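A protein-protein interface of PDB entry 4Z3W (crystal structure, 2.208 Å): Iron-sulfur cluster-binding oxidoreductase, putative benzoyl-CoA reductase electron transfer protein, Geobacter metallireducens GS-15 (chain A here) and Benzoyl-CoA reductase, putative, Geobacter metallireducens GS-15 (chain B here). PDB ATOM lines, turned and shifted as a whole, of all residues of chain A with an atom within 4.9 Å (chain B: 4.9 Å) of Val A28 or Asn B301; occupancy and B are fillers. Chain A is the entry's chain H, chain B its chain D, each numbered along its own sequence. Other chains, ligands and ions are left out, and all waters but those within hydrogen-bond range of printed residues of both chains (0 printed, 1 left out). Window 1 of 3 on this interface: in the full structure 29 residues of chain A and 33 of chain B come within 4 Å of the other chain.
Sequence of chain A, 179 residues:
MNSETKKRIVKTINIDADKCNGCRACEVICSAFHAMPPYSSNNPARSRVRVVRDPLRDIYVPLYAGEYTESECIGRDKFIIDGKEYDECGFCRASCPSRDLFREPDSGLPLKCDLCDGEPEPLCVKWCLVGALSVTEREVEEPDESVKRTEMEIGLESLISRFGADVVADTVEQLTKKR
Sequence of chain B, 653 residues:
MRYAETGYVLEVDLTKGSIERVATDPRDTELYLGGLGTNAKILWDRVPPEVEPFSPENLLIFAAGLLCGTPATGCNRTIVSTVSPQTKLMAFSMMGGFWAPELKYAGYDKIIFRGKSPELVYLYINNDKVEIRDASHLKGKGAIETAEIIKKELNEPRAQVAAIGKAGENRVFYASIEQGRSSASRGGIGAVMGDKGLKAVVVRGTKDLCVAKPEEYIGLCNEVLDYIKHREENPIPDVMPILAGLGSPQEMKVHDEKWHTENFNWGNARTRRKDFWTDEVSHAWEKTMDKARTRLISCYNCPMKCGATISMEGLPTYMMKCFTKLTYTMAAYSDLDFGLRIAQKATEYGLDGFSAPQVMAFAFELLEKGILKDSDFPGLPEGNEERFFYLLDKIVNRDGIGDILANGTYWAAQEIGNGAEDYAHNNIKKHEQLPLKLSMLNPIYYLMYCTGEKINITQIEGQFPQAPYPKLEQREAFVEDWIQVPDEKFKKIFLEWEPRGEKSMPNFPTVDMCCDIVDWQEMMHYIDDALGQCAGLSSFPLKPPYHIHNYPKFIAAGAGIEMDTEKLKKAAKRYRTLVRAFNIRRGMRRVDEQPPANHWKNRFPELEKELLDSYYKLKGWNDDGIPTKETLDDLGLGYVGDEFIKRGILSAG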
ATOM      1  N   CYS A  23     -11.627  20.088  23.398  1.00  0.00           N
ATOM      2  CA  CYS A  23     -10.471  19.528  24.104  1.00  0.00           C
ATOM      3  C   CYS A  23     -10.100  18.092  23.699  1.00  0.00           C
ATOM      4  O   CYS A  23      -8.968  17.665  23.904  1.00  0.00           O
ATOM      5  CB  CYS A  23     -10.728  19.571  25.612  1.00  0.00           C
ATOM      6  SG  CYS A  23     -11.981  18.422  26.242  1.00  0.00           S
ATOM      7  N   ARG A  24     -11.062  17.346  23.157  1.00  0.00           N
ATOM      8  CA  ARG A  24     -10.838  15.959  22.724  1.00  0.00           C
ATOM      9  C   ARG A  24     -10.528  14.981  23.871  1.00  0.00           C
ATOM     10  O   ARG A  24      -9.954  13.913  23.649  1.00  0.00           O
ATOM     11  CB  ARG A  24      -9.715  15.909  21.666  1.00  0.00           C
ATOM     12  CG  ARG A  24     -10.073  16.696  20.386  1.00  0.00           C
ATOM     13  CD  ARG A  24      -8.957  16.719  19.334  1.00  0.00           C
ATOM     14  NE  ARG A  24      -8.270  15.438  19.214  1.00  0.00           N
ATOM     15  CZ  ARG A  24      -6.998  15.318  18.838  1.00  0.00           C
ATOM     16  NH1 ARG A  24      -6.298  16.402  18.512  1.00  0.00           N
ATOM     17  NH2 ARG A  24      -6.431  14.120  18.774  1.00  0.00           N
ATOM     18  N   ALA A  25     -10.912  15.331  25.092  1.00  0.00           N
ATOM     19  CA  ALA A  25     -10.791  14.397  26.216  1.00  0.00           C
ATOM     20  C   ALA A  25     -11.598  13.129  25.949  1.00  0.00           C
ATOM     21  O   ALA A  25     -11.182  12.016  26.299  1.00  0.00           O
ATOM     22  CB  ALA A  25     -11.248  15.060  27.517  1.00  0.00           C
ATOM     23  N   CYS A  26     -12.754  13.299  25.308  1.00  0.00           N
ATOM     24  CA  CYS A  26     -13.589  12.156  24.923  1.00  0.00           C
ATOM     25  C   CYS A  26     -12.824  11.181  24.045  1.00  0.00           C
ATOM     26  O   CYS A  26     -12.916   9.961  24.238  1.00  0.00           O
ATOM     27  CB  CYS A  26     -14.857  12.628  24.211  1.00  0.00           C
ATOM     28  SG  CYS A  26     -14.606  14.041  23.132  1.00  0.00           S
ATOM     29  N   GLU A  27     -12.043  11.697  23.099  1.00  0.00           N
ATOM     30  CA  GLU A  27     -11.239  10.803  22.250  1.00  0.00           C
ATOM     31  C   GLU A  27     -10.176  10.085  23.051  1.00  0.00           C
ATOM     32  O   GLU A  27      -9.839   8.929  22.758  1.00  0.00           O
ATOM     33  CB  GLU A  27     -10.569  11.562  21.109  1.00  0.00           C
ATOM     34  CG  GLU A  27     -11.497  12.437  20.310  1.00  0.00           C
ATOM     35  CD  GLU A  27     -10.822  12.952  19.073  1.00  0.00           C
ATOM     36  OE1 GLU A  27      -9.577  12.865  19.035  1.00  0.00           O
ATOM     37  OE2 GLU A  27     -11.524  13.418  18.140  1.00  0.00           O
ATOM     38  N   VAL A  28      -9.631  10.781  24.054  1.00  0.00           N
ATOM     39  CA  VAL A  28      -8.560  10.216  24.860  1.00  0.00           C
ATOM     40  C   VAL A  28      -9.048   9.018  25.655  1.00  0.00           C
ATOM     41  O   VAL A  28      -8.405   7.963  25.677  1.00  0.00           O
ATOM     42  CB  VAL A  28      -7.979  11.240  25.861  1.00  0.00           C
ATOM     43  CG1 VAL A  28      -7.056  10.539  26.831  1.00  0.00           C
ATOM     44  CG2 VAL A  28      -7.263  12.373  25.130  1.00  0.00           C
ATOM     45  N   ILE A  29     -10.180   9.191  26.329  1.00  0.00           N
ATOM     46  CA  ILE A  29     -10.678   8.167  27.241  1.00  0.00           C
ATOM     47  C   ILE A  29     -11.382   7.010  26.510  1.00  0.00           C
ATOM     48  O   ILE A  29     -11.232   5.847  26.907  1.00  0.00           O
ATOM     49  CB  ILE A  29     -11.616   8.787  28.310  1.00  0.00           C
ATOM     50  CG1 ILE A  29     -11.958   7.748  29.374  1.00  0.00           C
ATOM     51  CG2 ILE A  29     -12.849   9.426  27.679  1.00  0.00           C
ATOM     52  CD1 ILE A  29     -10.767   7.377  30.246  1.00  0.00           C
ATOM     53  N   CYS A  30     -12.105   7.296  25.427  1.00  0.00           N
ATOM     54  CA  CYS A  30     -12.710   6.194  24.657  1.00  0.00           C
ATOM     55  C   CYS A  30     -11.607   5.291  24.087  1.00  0.00           C
ATOM     56  O   CYS A  30     -11.675   4.068  24.208  1.00  0.00           O
ATOM     57  CB  CYS A  30     -13.630   6.705  23.533  1.00  0.00           C
ATOM     58  SG  CYS A  30     -14.453   5.381  22.536  1.00  0.00           S
ATOM     59  N   SER A  31     -10.574   5.870  23.484  1.00  0.00           N
ATOM     60  CA  SER A  31      -9.508   5.020  22.937  1.00  0.00           C
ATOM     61  C   SER A  31      -8.773   4.289  24.063  1.00  0.00           C
ATOM     62  O   SER A  31      -8.470   3.100  23.950  1.00  0.00           O
ATOM     63  CB  SER A  31      -8.522   5.841  22.108  1.00  0.00           C
ATOM     64  OG  SER A  31      -8.067   6.964  22.839  1.00  0.00           O
ATOM     65  N   ALA A  32      -8.508   5.001  25.157  1.00  0.00           N
ATOM     66  CA  ALA A  32      -7.800   4.420  26.298  1.00  0.00           C
ATOM     67  C   ALA A  32      -8.564   3.225  26.859  1.00  0.00           C
ATOM     68  O   ALA A  32      -8.013   2.139  27.026  1.00  0.00           O
ATOM     69  CB  ALA A  32      -7.577   5.468  27.387  1.00  0.00           C
ATOM     70  N   ASN A  42      -3.479   4.740  24.690  1.00  0.00           N
ATOM     71  CA  ASN A  42      -4.561   5.491  24.065  1.00  0.00           C
ATOM     72  C   ASN A  42      -4.124   5.968  22.685  1.00  0.00           C
ATOM     73  O   ASN A  42      -2.947   5.862  22.333  1.00  0.00           O
ATOM     74  CB  ASN A  42      -4.997   6.664  24.945  1.00  0.00           C
ATOM     75  CG  ASN A  42      -4.127   7.887  24.765  1.00  0.00           C
ATOM     76  OD1 ASN A  42      -4.472   8.809  24.027  1.00  0.00           O
ATOM     77  ND2 ASN A  42      -2.998   7.902  25.439  1.00  0.00           N
ATOM     78  N   TRP A 127     -15.880  11.970  31.214  1.00  0.00           N
ATOM     79  CA  TRP A 127     -14.698  12.827  31.183  1.00  0.00           C
ATOM     80  C   TRP A 127     -14.998  14.192  30.592  1.00  0.00           C
ATOM     81  O   TRP A 127     -14.155  15.083  30.624  1.00  0.00           O
ATOM     82  CB  TRP A 127     -13.558  12.153  30.407  1.00  0.00           C
ATOM     83  CG  TRP A 127     -12.704  11.316  31.292  1.00  0.00           C
ATOM     84  CD1 TRP A 127     -13.116  10.574  32.359  1.00  0.00           C
ATOM     85  CD2 TRP A 127     -11.279  11.180  31.232  1.00  0.00           C
ATOM     86  NE1 TRP A 127     -12.039   9.963  32.956  1.00  0.00           N
ATOM     87  CE2 TRP A 127     -10.898  10.321  32.284  1.00  0.00           C
ATOM     88  CE3 TRP A 127     -10.292  11.687  30.385  1.00  0.00           C
ATOM     89  CZ2 TRP A 127      -9.575   9.958  32.507  1.00  0.00           C
ATOM     90  CZ3 TRP A 127      -8.973  11.328  30.615  1.00  0.00           C
ATOM     91  CH2 TRP A 127      -8.630  10.470  31.661  1.00  0.00           C
ATOM     92  N   THR B  70      -0.358  10.899  27.048  1.00  0.00           N
ATOM     93  CA  THR B  70      -1.047   9.986  27.956  1.00  0.00           C
ATOM     94  C   THR B  70      -2.359  10.623  28.337  1.00  0.00           C
ATOM     95  O   THR B  70      -2.598  11.787  28.013  1.00  0.00           O
ATOM     96  CB  THR B  70      -0.253   9.679  29.228  1.00  0.00           C
ATOM     97  OG1 THR B  70      -0.170  10.865  30.031  1.00  0.00           O
ATOM     98  CG2 THR B  70       1.139   9.168  28.883  1.00  0.00           C
ATOM     99  N   PRO B  71      -3.221   9.862  29.019  1.00  0.00           N
ATOM    100  CA  PRO B  71      -4.534  10.386  29.425  1.00  0.00           C
ATOM    101  C   PRO B  71      -4.512  11.471  30.511  1.00  0.00           C
ATOM    102  O   PRO B  71      -5.579  11.990  30.827  1.00  0.00           O
ATOM    103  CB  PRO B  71      -5.258   9.135  29.935  1.00  0.00           C
ATOM    104  CG  PRO B  71      -4.613   8.009  29.182  1.00  0.00           C
ATOM    105  CD  PRO B  71      -3.158   8.394  29.111  1.00  0.00           C
ATOM    106  N   ALA B  72      -3.347  11.827  31.049  1.00  0.00           N
ATOM    107  CA  ALA B  72      -3.276  12.834  32.124  1.00  0.00           C
ATOM    108  C   ALA B  72      -3.788  14.207  31.690  1.00  0.00           C
ATOM    109  O   ALA B  72      -3.287  14.797  30.738  1.00  0.00           O
ATOM    110  CB  ALA B  72      -1.839  12.961  32.649  1.00  0.00           C
ATOM    111  N   THR B  73      -4.778  14.710  32.417  1.00  0.00           N
ATOM    112  CA  THR B  73      -5.453  15.958  32.087  1.00  0.00           C
ATOM    113  C   THR B  73      -4.510  17.134  31.993  1.00  0.00           C
ATOM    114  O   THR B  73      -3.685  17.347  32.880  1.00  0.00           O
ATOM    115  CB  THR B  73      -6.512  16.301  33.134  1.00  0.00           C
ATOM    116  OG1 THR B  73      -7.364  15.168  33.346  1.00  0.00           O
ATOM    117  CG2 THR B  73      -7.327  17.490  32.688  1.00  0.00           C
ATOM    118  N   GLY B  74      -4.658  17.917  30.933  1.00  0.00           N
ATOM    119  CA  GLY B  74      -3.841  19.103  30.735  1.00  0.00           C
ATOM    120  C   GLY B  74      -2.383  18.849  30.379  1.00  0.00           C
ATOM    121  O   GLY B  74      -1.601  19.795  30.228  1.00  0.00           O
ATOM    122  N   TYR B 105       2.063  10.755  19.461  1.00  0.00           N
ATOM    123  CA  TYR B 105       1.289   9.806  18.647  1.00  0.00           C
ATOM    124  C   TYR B 105       1.950   9.542  17.292  1.00  0.00           C
ATOM    125  O   TYR B 105       1.676   8.523  16.645  1.00  0.00           O
ATOM    126  CB  TYR B 105      -0.141  10.309  18.411  1.00  0.00           C
ATOM    127  CG  TYR B 105      -0.964  10.473  19.662  1.00  0.00           C
ATOM    128  CD1 TYR B 105      -1.089   9.432  20.581  1.00  0.00           C
ATOM    129  CD2 TYR B 105      -1.610  11.678  19.935  1.00  0.00           C
ATOM    130  CE1 TYR B 105      -1.841   9.588  21.747  1.00  0.00           C
ATOM    131  CE2 TYR B 105      -2.352  11.853  21.103  1.00  0.00           C
ATOM    132  CZ  TYR B 105      -2.468  10.800  21.996  1.00  0.00           C
ATOM    133  OH  TYR B 105      -3.229  10.952  23.124  1.00  0.00           O
ATOM    134  N   CYS B 299      -6.983  23.642  25.686  1.00  0.00           N
ATOM    135  CA  CYS B 299      -5.912  22.866  25.088  1.00  0.00           C
ATOM    136  C   CYS B 299      -6.342  21.398  25.070  1.00  0.00           C
ATOM    137  O   CYS B 299      -7.444  21.065  25.501  1.00  0.00           O
ATOM    138  CB  CYS B 299      -4.596  23.037  25.854  1.00  0.00           C
ATOM    139  SG  CYS B 299      -4.102  24.736  26.032  1.00  0.00           S
ATOM    140  N   TYR B 300      -5.458  20.523  24.611  1.00  0.00           N
ATOM    141  CA  TYR B 300      -5.750  19.097  24.532  1.00  0.00           C
ATOM    142  C   TYR B 300      -6.065  18.501  25.895  1.00  0.00           C
ATOM    143  O   TYR B 300      -5.357  18.749  26.861  1.00  0.00           O
ATOM    144  CB  TYR B 300      -4.566  18.372  23.899  1.00  0.00           C
ATOM    145  CG  TYR B 300      -4.756  16.897  23.657  1.00  0.00           C
ATOM    146  CD1 TYR B 300      -5.714  16.433  22.756  1.00  0.00           C
ATOM    147  CD2 TYR B 300      -3.939  15.960  24.283  1.00  0.00           C
ATOM    148  CE1 TYR B 300      -5.873  15.074  22.506  1.00  0.00           C
ATOM    149  CE2 TYR B 300      -4.089  14.594  24.034  1.00  0.00           C
ATOM    150  CZ  TYR B 300      -5.063  14.162  23.146  1.00  0.00           C
ATOM    151  OH  TYR B 300      -5.218  12.812  22.901  1.00  0.00           O
ATOM    152  N   ASN B 301      -7.140  17.722  25.963  1.00  0.00           N
ATOM    153  CA  ASN B 301      -7.476  16.948  27.150  1.00  0.00           C
ATOM    154  C   ASN B 301      -7.603  17.796  28.416  1.00  0.00           C
ATOM    155  O   ASN B 301      -7.137  17.393  29.479  1.00  0.00           O
ATOM    156  CB  ASN B 301      -6.434  15.849  27.362  1.00  0.00           C
ATOM    157  CG  ASN B 301      -6.913  14.770  28.312  1.00  0.00           C
ATOM    158  OD1 ASN B 301      -8.114  14.598  28.504  1.00  0.00           O
ATOM    159  ND2 ASN B 301      -5.984  14.051  28.925  1.00  0.00           N
ATOM    160  N   CYS B 302      -8.248  18.959  28.308  1.00  0.00           N
ATOM    161  CA  CYS B 302      -8.432  19.835  29.473  1.00  0.00           C
ATOM    162  C   CYS B 302      -9.780  20.547  29.466  1.00  0.00           C
ATOM    163  O   CYS B 302     -10.215  21.065  28.436  1.00  0.00           O
ATOM    164  CB  CYS B 302      -7.318  20.883  29.551  1.00  0.00           C
ATOM    165  SG  CYS B 302      -7.272  21.854  31.112  1.00  0.00           S
ATOM    166  N   PRO B 303     -10.443  20.588  30.631  1.00  0.00           N
ATOM    167  CA  PRO B 303     -11.767  21.222  30.723  1.00  0.00           C
ATOM    168  C   PRO B 303     -11.749  22.696  31.092  1.00  0.00           C
ATOM    169  O   PRO B 303     -12.827  23.296  31.081  1.00  0.00           O
ATOM    170  CB  PRO B 303     -12.455  20.415  31.824  1.00  0.00           C
ATOM    171  CG  PRO B 303     -11.323  19.991  32.711  1.00  0.00           C
ATOM    172  CD  PRO B 303     -10.163  19.718  31.783  1.00  0.00           C
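The side-chain hydroxyl (OH) of Tyr B105 is in hydrogen-bond range of the side-chain amide oxygen (OD1) of Asn A42, at 2.6 Å. O of Cys A23 lies within hydrogen-bond range of N of Asn B301.
ND2 of Asn B301 lies within hydrogen-bond range of O of Pro B71, at 2.8 Å. O of Ala B72 sits at hydrogen-bond distance from ND2 of Asn B301. O of Asn B301 sits at hydrogen-bond distance from N of Gly B74. The side-chain hydroxyl (OH) of Tyr B300 is in hydrogen-bond range of the side-chain hydroxyl (OH) of Tyr B105, at 2.7 Å. SG of Cys A23 sits close to N of Ala A25 (3.5 Å). The side-chain carboxylate of Glu A27 lies within salt-bridge range of the guanidinium group of Arg A24 (2.9 Å).
Among the printed residues, pairs that only touch across the chains: Val A28 with Tyr B300 (3.1 Å), Cys A23 with Cys B302 (3.2 Å), Ala A25 with Asn B301 (3.3 Å), Trp A127 with Pro B71 (3.5 Å), Cys A23 with Tyr B300 (3.6 Å), Cys A23 with Cys B299 (3.6 Å), Val A28 with Pro B71 (3.6 Å), Asn A42 with Pro B71 (3.7 Å), Asn A42 with Thr B70 (3.8 Å), Arg A24 with Tyr B300 (3.8 Å), Trp A127 with Asn B301 (3.99 Å) and Val A28 with Asn B301 (3.999 Å).
Printed residues of chain B within 4 Å of Val A28: Pro B71 (3.6 Å), Tyr B300 (3.1 Å) and Asn B301 (3.999 Å). Printed residues of chain A within 4 Å of Asn B301: Cys A23, Ala A25, Val A28 and Trp A127. Of the printed residues of chain B, Asn A42 touches Thr B70, Pro B71 and Tyr B105. Of the printed residues of chain A, Cys B302 touches Cys A23. Ala B72 touches none of the printed residues of chain A. The nearest printed residue of chain A that does not touch Cys B299 is Arg A24 (5.7 Å).
Of the 12 printed residues of chain A, 6 touch a printed residue of chain B. Along chain A the printed residues that touch a printed residue of chain B span positions 23 to 127. Of the 11 printed residues of chain B, 7 touch a printed residue of chain A. Hydrophobic or aromatic side chains of chain B within 4 Å of the printed part of chain A: Pro B71, Tyr B105 and Tyr B300. Among the printed residues, no Asp or Glu carboxylate lies within 4 Å of a Lys or Arg side-chain nitrogen of the other chain.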
